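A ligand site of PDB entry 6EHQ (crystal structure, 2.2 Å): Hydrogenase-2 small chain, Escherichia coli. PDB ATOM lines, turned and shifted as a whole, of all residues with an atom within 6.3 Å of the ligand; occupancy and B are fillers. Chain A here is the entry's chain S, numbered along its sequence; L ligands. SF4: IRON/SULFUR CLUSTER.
An iron atom (FE3) of the ligand is bound by a ring nitrogen (ND1) of His 193 (2.1 Å).
The side-chain sulfur (SG) of Cys 221 binds an iron atom (FE1) of the ligand, 2.2 Å away.
An iron atom (FE4) of the ligand is bound by the side-chain sulfur (SG) of Cys 196 (2.3 Å).
SG of Cys 227 binds FE2 of the ligand (2.3 Å).
S3 of the ligand sits close to N of Leu 222 (3.5 Å).
The backbone NH (N) of Arg 199 lies close to a sulfur (S2) of the ligand.
O of His 193 is in hydrogen-bond range of NH1 of Arg 199 (3.1 Å).
The side-chain sulfur (SG) of Cys 221 sits close to the backbone NH (N) of Tyr 223 (3.3 Å).
The side-chain sulfur (SG) of Cys 196 lies close to the backbone NH (N) of Arg 198 (3.4 Å).
N of Cys 227 sits at hydrogen-bond distance from O of Leu 222, 3.3 Å away.
The side-chain sulfur (SG) of Cys 227 sits close to the backbone NH (N) of Gly 229 (3.4 Å).
SG of Cys 227 sits close to N of Cys 256.
The backbone carbonyl oxygen (O) of Val 250 sits at hydrogen-bond distance from the guanidinium group (NH2) of Arg 198 (3.3 Å).
The guanidinium group of Arg 198 sits at hydrogen-bond distance from the backbone carbonyl oxygen of Trp 220, 2.9 Å away.
S2 of the ligand lies close to O of Arg 198 (3.7 Å).
CB of Phe 202 touches S2 of the ligand, 3.98 Å away.
CB of Tyr 223 touches S4 of the ligand, at 3.7 Å.
CA of Gly 229 touches S1 of the ligand, at 3.8 Å.
Pro 230 touches the ligand (CD to S4, 3.97 Å).
CG1 of Val 250 touches S3 of the ligand, 3.9 Å away.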
ATOM      1  N   ILE A 192     -21.942 -34.917  28.136  1.00  0.00           N
ATOM      2  CA  ILE A 192     -23.257 -34.973  28.755  1.00  0.00           C
ATOM      3  C   ILE A 192     -24.276 -34.254  27.851  1.00  0.00           C
ATOM      4  O   ILE A 192     -25.400 -34.730  27.664  1.00  0.00           O
ATOM      5  CB  ILE A 192     -23.309 -34.319  30.172  1.00  0.00           C
ATOM      6  CG1 ILE A 192     -22.387 -34.938  31.201  1.00  0.00           C
ATOM      7  CG2 ILE A 192     -24.726 -34.361  30.742  1.00  0.00           C
ATOM      8  CD1 ILE A 192     -22.426 -36.417  31.236  1.00  0.00           C
ATOM      9  N   HIS A 193     -23.881 -33.092  27.312  1.00  0.00           N
ATOM     10  CA  HIS A 193     -24.722 -32.253  26.456  1.00  0.00           C
ATOM     11  C   HIS A 193     -25.057 -32.880  25.115  1.00  0.00           C
ATOM     12  O   HIS A 193     -26.017 -32.434  24.465  1.00  0.00           O
ATOM     13  CB  HIS A 193     -24.021 -30.928  26.280  1.00  0.00           C
ATOM     14  CG  HIS A 193     -24.727 -29.914  25.425  1.00  0.00           C
ATOM     15  ND1 HIS A 193     -25.820 -29.189  25.865  1.00  0.00           N
ATOM     16  CD2 HIS A 193     -24.424 -29.437  24.188  1.00  0.00           C
ATOM     17  CE1 HIS A 193     -26.166 -28.326  24.918  1.00  0.00           C
ATOM     18  NE2 HIS A 193     -25.334 -28.464  23.892  1.00  0.00           N
ATOM     19  N   GLU A 194     -24.275 -33.892  24.707  1.00  0.00           N
ATOM     20  CA  GLU A 194     -24.556 -34.645  23.489  1.00  0.00           C
ATOM     21  C   GLU A 194     -25.416 -35.877  23.735  1.00  0.00           C
ATOM     22  O   GLU A 194     -25.567 -36.725  22.856  1.00  0.00           O
ATOM     23  CB  GLU A 194     -23.262 -35.009  22.735  1.00  0.00           C
ATOM     24  CG  GLU A 194     -22.493 -33.786  22.175  1.00  0.00           C
ATOM     25  CD  GLU A 194     -23.321 -32.891  21.234  1.00  0.00           C
ATOM     26  OE1 GLU A 194     -23.557 -31.722  21.583  1.00  0.00           O
ATOM     27  OE2 GLU A 194     -23.750 -33.325  20.155  1.00  0.00           O
ATOM     28  N   CYS A 196     -28.247 -35.161  26.470  1.00  0.00           N
ATOM     29  CA  CYS A 196     -29.043 -34.611  27.529  1.00  0.00           C
ATOM     30  C   CYS A 196     -30.468 -34.392  27.081  1.00  0.00           C
ATOM     31  O   CYS A 196     -30.710 -33.799  26.044  1.00  0.00           O
ATOM     32  CB  CYS A 196     -28.474 -33.271  27.977  1.00  0.00           C
ATOM     33  SG  CYS A 196     -29.423 -32.489  29.317  1.00  0.00           S
ATOM     34  N   GLU A 197     -31.408 -34.844  27.920  1.00  0.00           N
ATOM     35  CA  GLU A 197     -32.838 -34.740  27.632  1.00  0.00           C
ATOM     36  C   GLU A 197     -33.378 -33.303  27.599  1.00  0.00           C
ATOM     37  O   GLU A 197     -34.468 -33.085  27.145  1.00  0.00           O
ATOM     38  CB  GLU A 197     -33.640 -35.604  28.611  1.00  0.00           C
ATOM     39  CG  GLU A 197     -33.721 -35.098  30.046  1.00  0.00           C
ATOM     40  CD  GLU A 197     -32.653 -35.663  30.973  1.00  0.00           C
ATOM     41  OE1 GLU A 197     -31.645 -36.273  30.474  1.00  0.00           O
ATOM     42  OE2 GLU A 197     -32.854 -35.489  32.211  1.00  0.00           O
ATOM     43  N   ARG A 198     -32.602 -32.339  28.073  1.00  0.00           N
ATOM     44  CA  ARG A 198     -32.965 -30.925  27.959  1.00  0.00           C
ATOM     45  C   ARG A 198     -32.435 -30.223  26.731  1.00  0.00           C
ATOM     46  O   ARG A 198     -32.662 -29.026  26.560  1.00  0.00           O
ATOM     47  CB  ARG A 198     -32.564 -30.192  29.239  1.00  0.00           C
ATOM     48  CG  ARG A 198     -33.220 -30.858  30.420  1.00  0.00           C
ATOM     49  CD  ARG A 198     -33.263 -29.971  31.623  1.00  0.00           C
ATOM     50  NE  ARG A 198     -33.963 -30.677  32.692  1.00  0.00           N
ATOM     51  CZ  ARG A 198     -34.375 -30.115  33.814  1.00  0.00           C
ATOM     52  NH1 ARG A 198     -34.201 -28.822  34.057  1.00  0.00           N
ATOM     53  NH2 ARG A 198     -34.985 -30.878  34.709  1.00  0.00           N
ATOM     54  N   ARG A 199     -31.799 -30.983  25.846  1.00  0.00           N
ATOM     55  CA  ARG A 199     -31.272 -30.427  24.601  1.00  0.00           C
ATOM     56  C   ARG A 199     -32.333 -29.740  23.754  1.00  0.00           C
ATOM     57  O   ARG A 199     -32.054 -28.688  23.169  1.00  0.00           O
ATOM     58  CB  ARG A 199     -30.489 -31.458  23.799  1.00  0.00           C
ATOM     59  CG  ARG A 199     -29.857 -30.930  22.516  1.00  0.00           C
ATOM     60  CD  ARG A 199     -28.834 -29.817  22.755  1.00  0.00           C
ATOM     61  NE  ARG A 199     -28.224 -29.545  21.457  1.00  0.00           N
ATOM     62  CZ  ARG A 199     -27.096 -30.099  20.996  1.00  0.00           C
ATOM     63  NH1 ARG A 199     -26.336 -30.922  21.740  1.00  0.00           N
ATOM     64  NH2 ARG A 199     -26.715 -29.815  19.765  1.00  0.00           N
ATOM     65  N   PRO A 200     -33.569 -30.298  23.710  1.00  0.00           N
ATOM     66  CA  PRO A 200     -34.607 -29.573  22.951  1.00  0.00           C
ATOM     67  C   PRO A 200     -34.847 -28.131  23.412  1.00  0.00           C
ATOM     68  O   PRO A 200     -35.138 -27.237  22.586  1.00  0.00           O
ATOM     69  CB  PRO A 200     -35.843 -30.434  23.169  1.00  0.00           C
ATOM     70  CG  PRO A 200     -35.297 -31.820  23.428  1.00  0.00           C
ATOM     71  CD  PRO A 200     -34.036 -31.608  24.164  1.00  0.00           C
ATOM     72  N   PHE A 202     -32.519 -26.221  25.100  1.00  0.00           N
ATOM     73  CA  PHE A 202     -31.341 -25.520  24.631  1.00  0.00           C
ATOM     74  C   PHE A 202     -31.555 -25.022  23.189  1.00  0.00           C
ATOM     75  O   PHE A 202     -31.412 -23.840  22.921  1.00  0.00           O
ATOM     76  CB  PHE A 202     -30.111 -26.421  24.725  1.00  0.00           C
ATOM     77  CG  PHE A 202     -28.802 -25.766  24.282  1.00  0.00           C
ATOM     78  CD1 PHE A 202     -28.409 -25.783  22.944  1.00  0.00           C
ATOM     79  CD2 PHE A 202     -27.973 -25.153  25.205  1.00  0.00           C
ATOM     80  CE1 PHE A 202     -27.222 -25.203  22.531  1.00  0.00           C
ATOM     81  CE2 PHE A 202     -26.771 -24.567  24.803  1.00  0.00           C
ATOM     82  CZ  PHE A 202     -26.402 -24.591  23.465  1.00  0.00           C
ATOM     83  N   PHE A 207     -34.623 -21.399  28.425  1.00  0.00           N
ATOM     84  CA  PHE A 207     -33.631 -21.489  29.498  1.00  0.00           C
ATOM     85  C   PHE A 207     -34.197 -21.068  30.835  1.00  0.00           C
ATOM     86  O   PHE A 207     -34.909 -20.106  30.896  1.00  0.00           O
ATOM     87  CB  PHE A 207     -32.481 -20.563  29.200  1.00  0.00           C
ATOM     88  CG  PHE A 207     -31.763 -20.878  27.917  1.00  0.00           C
ATOM     89  CD1 PHE A 207     -30.958 -22.015  27.813  1.00  0.00           C
ATOM     90  CD2 PHE A 207     -31.832 -20.005  26.823  1.00  0.00           C
ATOM     91  CE1 PHE A 207     -30.262 -22.283  26.656  1.00  0.00           C
ATOM     92  CE2 PHE A 207     -31.133 -20.270  25.642  1.00  0.00           C
ATOM     93  CZ  PHE A 207     -30.345 -21.417  25.551  1.00  0.00           C
ATOM     94  N   TRP A 220     -36.760 -26.561  31.946  1.00  0.00           N
ATOM     95  CA  TRP A 220     -36.003 -26.066  30.816  1.00  0.00           C
ATOM     96  C   TRP A 220     -34.493 -26.271  31.001  1.00  0.00           C
ATOM     97  O   TRP A 220     -34.005 -26.732  32.075  1.00  0.00           O
ATOM     98  CB  TRP A 220     -36.348 -24.602  30.541  1.00  0.00           C
ATOM     99  CG  TRP A 220     -37.755 -24.370  30.011  1.00  0.00           C
ATOM    100  CD1 TRP A 220     -38.682 -25.330  29.681  1.00  0.00           C
ATOM    101  CD2 TRP A 220     -38.385 -23.107  29.704  1.00  0.00           C
ATOM    102  NE1 TRP A 220     -39.824 -24.758  29.200  1.00  0.00           N
ATOM    103  CE2 TRP A 220     -39.668 -23.389  29.195  1.00  0.00           C
ATOM    104  CE3 TRP A 220     -37.974 -21.768  29.781  1.00  0.00           C
ATOM    105  CZ2 TRP A 220     -40.576 -22.380  28.805  1.00  0.00           C
ATOM    106  CZ3 TRP A 220     -38.867 -20.753  29.402  1.00  0.00           C
ATOM    107  CH2 TRP A 220     -40.170 -21.082  28.912  1.00  0.00           C
ATOM    108  N   CYS A 221     -33.734 -25.955  29.954  1.00  0.00           N
ATOM    109  CA  CYS A 221     -32.292 -26.144  29.957  1.00  0.00           C
ATOM    110  C   CYS A 221     -31.606 -25.235  30.970  1.00  0.00           C
ATOM    111  O   CYS A 221     -31.983 -24.080  31.145  1.00  0.00           O
ATOM    112  CB  CYS A 221     -31.720 -25.887  28.559  1.00  0.00           C
ATOM    113  SG  CYS A 221     -29.905 -25.793  28.416  1.00  0.00           S
ATOM    114  N   LEU A 222     -30.549 -25.776  31.599  1.00  0.00           N
ATOM    115  CA  LEU A 222     -29.850 -25.101  32.658  1.00  0.00           C
ATOM    116  C   LEU A 222     -28.560 -24.377  32.219  1.00  0.00           C
ATOM    117  O   LEU A 222     -27.776 -23.919  33.061  1.00  0.00           O
ATOM    118  CB  LEU A 222     -29.576 -26.123  33.757  1.00  0.00           C
ATOM    119  CG  LEU A 222     -30.809 -26.882  34.281  1.00  0.00           C
ATOM    120  CD1 LEU A 222     -30.504 -27.750  35.514  1.00  0.00           C
ATOM    121  CD2 LEU A 222     -31.937 -25.909  34.624  1.00  0.00           C
ATOM    122  N   TYR A 223     -28.349 -24.255  30.902  1.00  0.00           N
ATOM    123  CA  TYR A 223     -27.146 -23.629  30.353  1.00  0.00           C
ATOM    124  C   TYR A 223     -26.859 -22.287  31.015  1.00  0.00           C
ATOM    125  O   TYR A 223     -25.736 -22.052  31.483  1.00  0.00           O
ATOM    126  CB  TYR A 223     -27.228 -23.447  28.812  1.00  0.00           C
ATOM    127  CG  TYR A 223     -25.992 -22.801  28.278  1.00  0.00           C
ATOM    128  CD1 TYR A 223     -24.792 -23.515  28.217  1.00  0.00           C
ATOM    129  CD2 TYR A 223     -25.982 -21.443  27.911  1.00  0.00           C
ATOM    130  CE1 TYR A 223     -23.615 -22.928  27.778  1.00  0.00           C
ATOM    131  CE2 TYR A 223     -24.818 -20.814  27.482  1.00  0.00           C
ATOM    132  CZ  TYR A 223     -23.630 -21.554  27.418  1.00  0.00           C
ATOM    133  OH  TYR A 223     -22.459 -20.949  27.011  1.00  0.00           O
ATOM    134  N   HIS A 224     -27.873 -21.425  31.096  1.00  0.00           N
ATOM    135  CA  HIS A 224     -27.683 -20.071  31.652  1.00  0.00           C
ATOM    136  C   HIS A 224     -27.530 -19.998  33.166  1.00  0.00           C
ATOM    137  O   HIS A 224     -27.206 -18.928  33.670  1.00  0.00           O
ATOM    138  CB  HIS A 224     -28.692 -19.068  31.065  1.00  0.00           C
ATOM    139  CG  HIS A 224     -28.295 -18.619  29.685  1.00  0.00           C
ATOM    140  ND1 HIS A 224     -27.219 -17.762  29.454  1.00  0.00           N
ATOM    141  CD2 HIS A 224     -28.742 -18.994  28.471  1.00  0.00           C
ATOM    142  CE1 HIS A 224     -27.103 -17.576  28.156  1.00  0.00           C
ATOM    143  NE2 HIS A 224     -27.996 -18.318  27.533  1.00  0.00           N
ATOM    144  N   CYS A 227     -24.550 -24.605  33.423  1.00  0.00           N
ATOM    145  CA  CYS A 227     -24.418 -26.027  33.164  1.00  0.00           C
ATOM    146  C   CYS A 227     -23.178 -26.324  32.372  1.00  0.00           C
ATOM    147  O   CYS A 227     -22.989 -25.776  31.299  1.00  0.00           O
ATOM    148  CB  CYS A 227     -25.658 -26.600  32.466  1.00  0.00           C
ATOM    149  SG  CYS A 227     -25.594 -28.399  32.302  1.00  0.00           S
ATOM    150  N   LYS A 228     -22.323 -27.195  32.912  1.00  0.00           N
ATOM    151  CA  LYS A 228     -21.081 -27.585  32.260  1.00  0.00           C
ATOM    152  C   LYS A 228     -21.223 -28.841  31.426  1.00  0.00           C
ATOM    153  O   LYS A 228     -20.210 -29.392  30.959  1.00  0.00           O
ATOM    154  CB  LYS A 228     -19.977 -27.827  33.304  1.00  0.00           C
ATOM    155  CG  LYS A 228     -19.737 -26.673  34.242  1.00  0.00           C
ATOM    156  CD  LYS A 228     -19.544 -25.370  33.488  1.00  0.00           C
ATOM    157  CE  LYS A 228     -19.011 -24.286  34.394  1.00  0.00           C
ATOM    158  NZ  LYS A 228     -19.989 -23.998  35.493  1.00  0.00           N
ATOM    159  N   GLY A 229     -22.458 -29.330  31.218  1.00  0.00           N
ATOM    160  CA  GLY A 229     -22.672 -30.455  30.318  1.00  0.00           C
ATOM    161  C   GLY A 229     -21.973 -30.328  28.948  1.00  0.00           C
ATOM    162  O   GLY A 229     -21.495 -31.319  28.405  1.00  0.00           O
ATOM    163  N   PRO A 230     -21.935 -29.108  28.394  1.00  0.00           N
ATOM    164  CA  PRO A 230     -21.297 -28.976  27.067  1.00  0.00           C
ATOM    165  C   PRO A 230     -19.803 -29.253  26.999  1.00  0.00           C
ATOM    166  O   PRO A 230     -19.296 -29.399  25.918  1.00  0.00           O
ATOM    167  CB  PRO A 230     -21.577 -27.527  26.681  1.00  0.00           C
ATOM    168  CG  PRO A 230     -22.835 -27.212  27.398  1.00  0.00           C
ATOM    169  CD  PRO A 230     -22.733 -27.924  28.706  1.00  0.00           C
ATOM    170  N   TRP A 248     -30.355 -37.299  38.417  1.00  0.00           N
ATOM    171  CA  TRP A 248     -29.018 -36.767  38.236  1.00  0.00           C
ATOM    172  C   TRP A 248     -29.139 -35.265  38.506  1.00  0.00           C
ATOM    173  O   TRP A 248     -30.254 -34.787  38.693  1.00  0.00           O
ATOM    174  CB  TRP A 248     -28.432 -37.124  36.854  1.00  0.00           C
ATOM    175  CG  TRP A 248     -29.072 -36.536  35.610  1.00  0.00           C
ATOM    176  CD1 TRP A 248     -30.336 -36.765  35.117  1.00  0.00           C
ATOM    177  CD2 TRP A 248     -28.444 -35.657  34.661  1.00  0.00           C
ATOM    178  NE1 TRP A 248     -30.537 -36.081  33.937  1.00  0.00           N
ATOM    179  CE2 TRP A 248     -29.398 -35.391  33.632  1.00  0.00           C
ATOM    180  CE3 TRP A 248     -27.188 -35.066  34.572  1.00  0.00           C
ATOM    181  CZ2 TRP A 248     -29.105 -34.562  32.540  1.00  0.00           C
ATOM    182  CZ3 TRP A 248     -26.898 -34.240  33.504  1.00  0.00           C
ATOM    183  CH2 TRP A 248     -27.860 -34.005  32.485  1.00  0.00           C
ATOM    184  N   VAL A 250     -28.939 -32.378  36.871  1.00  0.00           N
ATOM    185  CA  VAL A 250     -29.796 -31.585  35.992  1.00  0.00           C
ATOM    186  C   VAL A 250     -31.258 -31.940  36.150  1.00  0.00           C
ATOM    187  O   VAL A 250     -32.105 -31.053  36.223  1.00  0.00           O
ATOM    188  CB  VAL A 250     -29.351 -31.694  34.550  1.00  0.00           C
ATOM    189  CG1 VAL A 250     -30.406 -31.112  33.615  1.00  0.00           C
ATOM    190  CG2 VAL A 250     -28.005 -31.003  34.372  1.00  0.00           C
ATOM    191  N   PRO A 255     -27.495 -27.203  37.657  1.00  0.00           N
ATOM    192  CA  PRO A 255     -26.601 -27.424  36.525  1.00  0.00           C
ATOM    193  C   PRO A 255     -25.478 -28.422  36.836  1.00  0.00           C
ATOM    194  O   PRO A 255     -25.152 -28.638  38.002  1.00  0.00           O
ATOM    195  CB  PRO A 255     -26.040 -26.027  36.231  1.00  0.00           C
ATOM    196  CG  PRO A 255     -26.306 -25.239  37.451  1.00  0.00           C
ATOM    197  CD  PRO A 255     -27.569 -25.776  38.012  1.00  0.00           C
ATOM    198  N   CYS A 256     -24.987 -29.082  35.787  1.00  0.00           N
ATOM    199  CA  CYS A 256     -23.765 -29.867  35.880  1.00  0.00           C
ATOM    200  C   CYS A 256     -22.642 -28.881  36.198  1.00  0.00           C
ATOM    201  O   CYS A 256     -22.628 -27.753  35.675  1.00  0.00           O
ATOM    202  CB  CYS A 256     -23.482 -30.612  34.577  1.00  0.00           C
ATOM    203  SG  CYS A 256     -21.887 -31.468  34.459  1.00  0.00           S
HETATM  204 FE1  SF4 L   1     -28.852 -27.704  28.795  1.00  0.00          FE
HETATM  205 FE2  SF4 L   1     -26.849 -28.689  30.389  1.00  0.00          FE
HETATM  206 FE3  SF4 L   1     -26.729 -29.038  27.705  1.00  0.00          FE
HETATM  207 FE4  SF4 L   1     -28.584 -30.386  29.164  1.00  0.00          FE
HETATM  208  S1  SF4 L   1     -26.283 -30.604  29.273  1.00  0.00           S
HETATM  209  S2  SF4 L   1     -28.996 -29.313  27.217  1.00  0.00           S
HETATM  210  S3  SF4 L   1     -29.119 -28.840  30.748  1.00  0.00           S
HETATM  211  S4  SF4 L   1     -26.609 -27.069  28.793  1.00  0.00           S
